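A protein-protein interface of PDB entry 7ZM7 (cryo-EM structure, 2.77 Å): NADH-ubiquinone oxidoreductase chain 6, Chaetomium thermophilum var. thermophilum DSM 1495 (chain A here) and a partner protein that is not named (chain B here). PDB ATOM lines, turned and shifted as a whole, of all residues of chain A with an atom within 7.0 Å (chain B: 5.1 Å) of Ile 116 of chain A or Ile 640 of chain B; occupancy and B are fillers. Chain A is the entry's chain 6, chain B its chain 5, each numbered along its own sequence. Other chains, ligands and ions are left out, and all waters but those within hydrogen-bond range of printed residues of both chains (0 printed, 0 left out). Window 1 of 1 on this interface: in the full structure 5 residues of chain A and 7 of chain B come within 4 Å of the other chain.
O of Ile 116 of chain A sits at hydrogen-bond distance from OG of Ser 119 of chain A (3.1 Å).
Among the printed residues, pairs that only touch across the chains: Phe 120 of chain A with Leu 643 of chain B (3.3 Å), Ile 117 of chain A with Ile 640 of chain B (3.6 Å), Ile 116 of chain A with Ile 640 of chain B (3.7 Å), Phe 120 of chain A with Ile 644 of chain B (3.7 Å) and Val 113 of chain A with Leu 636 of chain B (3.9 Å).
Ile 116 of chain A touches one residue of chain B.
Ile 640 of chain B touches just these residues of chain A: Ile 116 (3.7 Å) and Ile 117 (3.6 Å).
Of the printed residues of chain A, Ile 644 of chain B touches Phe 120.
Of the printed residues of chain A, Leu 636 of chain B touches Val 113.
Printed residues of chain B within 4 Å of Ile 117 of chain A: Ile 640.
Of the printed residues of chain A, Leu 643 of chain B touches Phe 120 (3.3 Å).
Leu 112 of chain A touches none of the printed residues of chain B.
Val 637 of chain B touches none of the printed residues of chain A.
The nearest residue of chain B that does not touch Ile 116 of chain A is Ile 644 of chain B (4.1 Å).
The nearest residue of chain A that does not touch Ile 640 of chain B is Val 113 of chain A (4.04 Å).
Of the 10 printed residues of chain B, 4 touch a printed residue of chain A.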
ATOM      1  N   ILE A 111      12.882   8.490  -2.760  1.00  0.00           N
ATOM      2  CA  ILE A 111      12.763   9.898  -2.399  1.00  0.00           C
ATOM      3  C   ILE A 111      14.041  10.646  -2.744  1.00  0.00           C
ATOM      4  O   ILE A 111      14.006  11.742  -3.316  1.00  0.00           O
ATOM      5  CB  ILE A 111      12.419  10.034  -0.904  1.00  0.00           C
ATOM      6  CG1 ILE A 111      11.029   9.468  -0.625  1.00  0.00           C
ATOM      7  CG2 ILE A 111      12.487  11.482  -0.473  1.00  0.00           C
ATOM      8  CD1 ILE A 111      10.754   9.233   0.842  1.00  0.00           C
ATOM      9  N   LEU A 112      15.192  10.059  -2.416  1.00  0.00           N
ATOM     10  CA  LEU A 112      16.461  10.753  -2.590  1.00  0.00           C
ATOM     11  C   LEU A 112      16.802  10.934  -4.062  1.00  0.00           C
ATOM     12  O   LEU A 112      17.139  12.039  -4.500  1.00  0.00           O
ATOM     13  CB  LEU A 112      17.566   9.987  -1.869  1.00  0.00           C
ATOM     14  CG  LEU A 112      17.500  10.117  -0.348  1.00  0.00           C
ATOM     15  CD1 LEU A 112      18.711   9.479   0.310  1.00  0.00           C
ATOM     16  CD2 LEU A 112      17.373  11.575   0.061  1.00  0.00           C
ATOM     17  N   VAL A 113      16.710   9.863  -4.847  1.00  0.00           N
ATOM     18  CA  VAL A 113      17.150   9.939  -6.235  1.00  0.00           C
ATOM     19  C   VAL A 113      16.151  10.729  -7.078  1.00  0.00           C
ATOM     20  O   VAL A 113      16.508  11.308  -8.107  1.00  0.00           O
ATOM     21  CB  VAL A 113      17.397   8.525  -6.789  1.00  0.00           C
ATOM     22  CG1 VAL A 113      17.898   8.591  -8.225  1.00  0.00           C
ATOM     23  CG2 VAL A 113      18.394   7.807  -5.912  1.00  0.00           C
ATOM     24  N   GLY A 114      14.892  10.771  -6.657  1.00  0.00           N
ATOM     25  CA  GLY A 114      13.922  11.584  -7.369  1.00  0.00           C
ATOM     26  C   GLY A 114      14.214  13.070  -7.280  1.00  0.00           C
ATOM     27  O   GLY A 114      14.038  13.807  -8.251  1.00  0.00           O
ATOM     28  N   ILE A 115      14.653  13.534  -6.111  1.00  0.00           N
ATOM     29  CA  ILE A 115      14.943  14.953  -5.952  1.00  0.00           C
ATOM     30  C   ILE A 115      16.198  15.342  -6.723  1.00  0.00           C
ATOM     31  O   ILE A 115      16.226  16.365  -7.417  1.00  0.00           O
ATOM     32  CB  ILE A 115      15.063  15.299  -4.458  1.00  0.00           C
ATOM     33  CG1 ILE A 115      13.674  15.408  -3.833  1.00  0.00           C
ATOM     34  CG2 ILE A 115      15.842  16.578  -4.263  1.00  0.00           C
ATOM     35  CD1 ILE A 115      13.691  15.478  -2.325  1.00  0.00           C
ATOM     36  N   ILE A 116      17.252  14.533  -6.623  1.00  0.00           N
ATOM     37  CA  ILE A 116      18.545  14.913  -7.182  1.00  0.00           C
ATOM     38  C   ILE A 116      18.498  14.935  -8.706  1.00  0.00           C
ATOM     39  O   ILE A 116      18.972  15.885  -9.339  1.00  0.00           O
ATOM     40  CB  ILE A 116      19.643  13.968  -6.670  1.00  0.00           C
ATOM     41  CG1 ILE A 116      19.771  14.071  -5.154  1.00  0.00           C
ATOM     42  CG2 ILE A 116      20.966  14.291  -7.336  1.00  0.00           C
ATOM     43  CD1 ILE A 116      20.412  12.858  -4.527  1.00  0.00           C
ATOM     44  N   ILE A 117      17.946  13.888  -9.323  1.00  0.00           N
ATOM     45  CA  ILE A 117      17.866  13.871 -10.780  1.00  0.00           C
ATOM     46  C   ILE A 117      16.946  14.975 -11.282  1.00  0.00           C
ATOM     47  O   ILE A 117      17.279  15.693 -12.231  1.00  0.00           O
ATOM     48  CB  ILE A 117      17.429  12.491 -11.301  1.00  0.00           C
ATOM     49  CG1 ILE A 117      18.567  11.488 -11.163  1.00  0.00           C
ATOM     50  CG2 ILE A 117      17.005  12.580 -12.754  1.00  0.00           C
ATOM     51  CD1 ILE A 117      18.192  10.104 -11.568  1.00  0.00           C
ATOM     52  N   SER A 118      15.783  15.135 -10.651  1.00  0.00           N
ATOM     53  CA  SER A 118      14.838  16.140 -11.122  1.00  0.00           C
ATOM     54  C   SER A 118      15.421  17.542 -11.012  1.00  0.00           C
ATOM     55  O   SER A 118      15.255  18.363 -11.921  1.00  0.00           O
ATOM     56  CB  SER A 118      13.537  16.046 -10.337  1.00  0.00           C
ATOM     57  OG  SER A 118      13.741  16.431  -8.991  1.00  0.00           O
ATOM     58  N   SER A 119      16.113  17.836  -9.910  1.00  0.00           N
ATOM     59  CA  SER A 119      16.626  19.186  -9.712  1.00  0.00           C
ATOM     60  C   SER A 119      17.726  19.529 -10.708  1.00  0.00           C
ATOM     61  O   SER A 119      17.872  20.698 -11.082  1.00  0.00           O
ATOM     62  CB  SER A 119      17.138  19.356  -8.284  1.00  0.00           C
ATOM     63  OG  SER A 119      18.337  18.631  -8.083  1.00  0.00           O
ATOM     64  N   PHE A 120      18.509  18.541 -11.142  1.00  0.00           N
ATOM     65  CA  PHE A 120      19.605  18.825 -12.066  1.00  0.00           C
ATOM     66  C   PHE A 120      19.131  18.838 -13.511  1.00  0.00           C
ATOM     67  O   PHE A 120      19.274  19.845 -14.211  1.00  0.00           O
ATOM     68  CB  PHE A 120      20.728  17.803 -11.898  1.00  0.00           C
ATOM     69  CG  PHE A 120      21.584  18.042 -10.706  1.00  0.00           C
ATOM     70  CD1 PHE A 120      21.477  19.215  -9.990  1.00  0.00           C
ATOM     71  CD2 PHE A 120      22.506  17.095 -10.304  1.00  0.00           C
ATOM     72  CE1 PHE A 120      22.268  19.438  -8.888  1.00  0.00           C
ATOM     73  CE2 PHE A 120      23.301  17.311  -9.207  1.00  0.00           C
ATOM     74  CZ  PHE A 120      23.183  18.485  -8.498  1.00  0.00           C
ATOM     75  N   LEU A 121      18.561  17.725 -13.972  1.00  0.00           N
ATOM     76  CA  LEU A 121      18.249  17.589 -15.390  1.00  0.00           C
ATOM     77  C   LEU A 121      17.284  18.662 -15.872  1.00  0.00           C
ATOM     78  O   LEU A 121      17.365  19.084 -17.029  1.00  0.00           O
ATOM     79  CB  LEU A 121      17.677  16.204 -15.673  1.00  0.00           C
ATOM     80  CG  LEU A 121      18.658  15.142 -16.166  1.00  0.00           C
ATOM     81  CD1 LEU A 121      18.041  13.761 -16.062  1.00  0.00           C
ATOM     82  CD2 LEU A 121      19.069  15.433 -17.598  1.00  0.00           C
ATOM     83  N   LEU B 636      23.832   3.668 -10.877  1.00  0.00           N
ATOM     84  CA  LEU B 636      23.011   4.884 -10.661  1.00  0.00           C
ATOM     85  C   LEU B 636      23.555   5.614  -9.441  1.00  0.00           C
ATOM     86  O   LEU B 636      23.610   6.850  -9.469  1.00  0.00           O
ATOM     87  CB  LEU B 636      21.568   4.424 -10.461  1.00  0.00           C
ATOM     88  CG  LEU B 636      20.521   5.457 -10.064  1.00  0.00           C
ATOM     89  CD1 LEU B 636      19.186   5.047 -10.649  1.00  0.00           C
ATOM     90  CD2 LEU B 636      20.401   5.560  -8.549  1.00  0.00           C
ATOM     91  N   VAL B 637      23.961   4.869  -8.416  1.00  0.00           N
ATOM     92  CA  VAL B 637      24.568   5.539  -7.275  1.00  0.00           C
ATOM     93  C   VAL B 637      25.828   6.261  -7.710  1.00  0.00           C
ATOM     94  O   VAL B 637      26.031   7.434  -7.391  1.00  0.00           O
ATOM     95  CB  VAL B 637      24.855   4.534  -6.146  1.00  0.00           C
ATOM     96  CG1 VAL B 637      25.723   5.175  -5.077  1.00  0.00           C
ATOM     97  CG2 VAL B 637      23.560   4.042  -5.550  1.00  0.00           C
ATOM     98  N   GLY B 638      26.677   5.578  -8.475  1.00  0.00           N
ATOM     99  CA  GLY B 638      27.881   6.209  -8.985  1.00  0.00           C
ATOM    100  C   GLY B 638      27.601   7.312  -9.980  1.00  0.00           C
ATOM    101  O   GLY B 638      28.439   8.184 -10.193  1.00  0.00           O
ATOM    102  N   PHE B 639      26.436   7.278 -10.618  1.00  0.00           N
ATOM    103  CA  PHE B 639      26.019   8.389 -11.467  1.00  0.00           C
ATOM    104  C   PHE B 639      25.601   9.606 -10.652  1.00  0.00           C
ATOM    105  O   PHE B 639      25.962  10.730 -10.996  1.00  0.00           O
ATOM    106  CB  PHE B 639      24.912   7.929 -12.406  1.00  0.00           C
ATOM    107  CG  PHE B 639      24.570   8.919 -13.479  1.00  0.00           C
ATOM    108  CD1 PHE B 639      25.474   9.228 -14.476  1.00  0.00           C
ATOM    109  CD2 PHE B 639      23.370   9.615 -13.437  1.00  0.00           C
ATOM    110  CE1 PHE B 639      25.162  10.155 -15.458  1.00  0.00           C
ATOM    111  CE2 PHE B 639      23.052  10.529 -14.406  1.00  0.00           C
ATOM    112  CZ  PHE B 639      23.946  10.807 -15.414  1.00  0.00           C
ATOM    113  N   ILE B 640      24.856   9.408  -9.568  1.00  0.00           N
ATOM    114  CA  ILE B 640      24.386  10.543  -8.783  1.00  0.00           C
ATOM    115  C   ILE B 640      25.556  11.299  -8.174  1.00  0.00           C
ATOM    116  O   ILE B 640      25.593  12.535  -8.185  1.00  0.00           O
ATOM    117  CB  ILE B 640      23.399  10.072  -7.705  1.00  0.00           C
ATOM    118  CG1 ILE B 640      22.204   9.378  -8.349  1.00  0.00           C
ATOM    119  CG2 ILE B 640      22.971  11.233  -6.822  1.00  0.00           C
ATOM    120  CD1 ILE B 640      21.417  10.266  -9.275  1.00  0.00           C
ATOM    121  N   LEU B 641      26.532  10.572  -7.641  1.00  0.00           N
ATOM    122  CA  LEU B 641      27.668  11.218  -7.003  1.00  0.00           C
ATOM    123  C   LEU B 641      28.452  12.064  -7.997  1.00  0.00           C
ATOM    124  O   LEU B 641      28.999  13.110  -7.634  1.00  0.00           O
ATOM    125  CB  LEU B 641      28.552  10.158  -6.353  1.00  0.00           C
ATOM    126  CG  LEU B 641      27.764   9.218  -5.444  1.00  0.00           C
ATOM    127  CD1 LEU B 641      28.512   7.931  -5.185  1.00  0.00           C
ATOM    128  CD2 LEU B 641      27.449   9.917  -4.136  1.00  0.00           C
ATOM    129  N   TYR B 642      28.532  11.623  -9.254  1.00  0.00           N
ATOM    130  CA  TYR B 642      29.204  12.428 -10.269  1.00  0.00           C
ATOM    131  C   TYR B 642      28.443  13.709 -10.550  1.00  0.00           C
ATOM    132  O   TYR B 642      29.047  14.771 -10.708  1.00  0.00           O
ATOM    133  CB  TYR B 642      29.384  11.628 -11.555  1.00  0.00           C
ATOM    134  CG  TYR B 642      30.619  10.778 -11.550  1.00  0.00           C
ATOM    135  CD1 TYR B 642      30.960  10.033 -10.445  1.00  0.00           C
ATOM    136  CD2 TYR B 642      31.447  10.728 -12.640  1.00  0.00           C
ATOM    137  CE1 TYR B 642      32.079   9.255 -10.442  1.00  0.00           C
ATOM    138  CE2 TYR B 642      32.563   9.948 -12.648  1.00  0.00           C
ATOM    139  CZ  TYR B 642      32.880   9.224 -11.554  1.00  0.00           C
ATOM    140  OH  TYR B 642      34.011   8.451 -11.563  1.00  0.00           O
ATOM    141  N   LEU B 643      27.121  13.623 -10.636  1.00  0.00           N
ATOM    142  CA  LEU B 643      26.303  14.808 -10.855  1.00  0.00           C
ATOM    143  C   LEU B 643      26.378  15.759  -9.676  1.00  0.00           C
ATOM    144  O   LEU B 643      26.523  16.971  -9.859  1.00  0.00           O
ATOM    145  CB  LEU B 643      24.859  14.400 -11.131  1.00  0.00           C
ATOM    146  CG  LEU B 643      24.500  14.003 -12.560  1.00  0.00           C
ATOM    147  CD1 LEU B 643      24.686  15.211 -13.436  1.00  0.00           C
ATOM    148  CD2 LEU B 643      25.349  12.888 -13.081  1.00  0.00           C
ATOM    149  N   ILE B 644      26.290  15.232  -8.458  1.00  0.00           N
ATOM    150  CA  ILE B 644      26.438  16.078  -7.283  1.00  0.00           C
ATOM    151  C   ILE B 644      27.797  16.746  -7.278  1.00  0.00           C
ATOM    152  O   ILE B 644      27.906  17.962  -7.099  1.00  0.00           O
ATOM    153  CB  ILE B 644      26.205  15.263  -6.001  1.00  0.00           C
ATOM    154  CG1 ILE B 644      24.723  14.915  -5.863  1.00  0.00           C
ATOM    155  CG2 ILE B 644      26.723  16.009  -4.800  1.00  0.00           C
ATOM    156  CD1 ILE B 644      24.443  13.928  -4.768  1.00  0.00           C
ATOM    157  N   TYR B 645      28.853  15.975  -7.513  1.00  0.00           N
ATOM    158  CA  TYR B 645      30.192  16.543  -7.458  1.00  0.00           C
ATOM    159  C   TYR B 645      30.354  17.689  -8.438  1.00  0.00           C
ATOM    160  O   TYR B 645      30.787  18.782  -8.063  1.00  0.00           O
ATOM    161  CB  TYR B 645      31.227  15.466  -7.731  1.00  0.00           C
ATOM    162  CG  TYR B 645      32.626  16.003  -7.754  1.00  0.00           C
ATOM    163  CD1 TYR B 645      33.322  16.238  -6.580  1.00  0.00           C
ATOM    164  CD2 TYR B 645      33.250  16.286  -8.956  1.00  0.00           C
ATOM    165  CE1 TYR B 645      34.605  16.734  -6.604  1.00  0.00           C
ATOM    166  CE2 TYR B 645      34.526  16.779  -8.991  1.00  0.00           C
ATOM    167  CZ  TYR B 645      35.203  17.003  -7.814  1.00  0.00           C
ATOM    168  OH  TYR B 645      36.482  17.501  -7.857  1.00  0.00           O
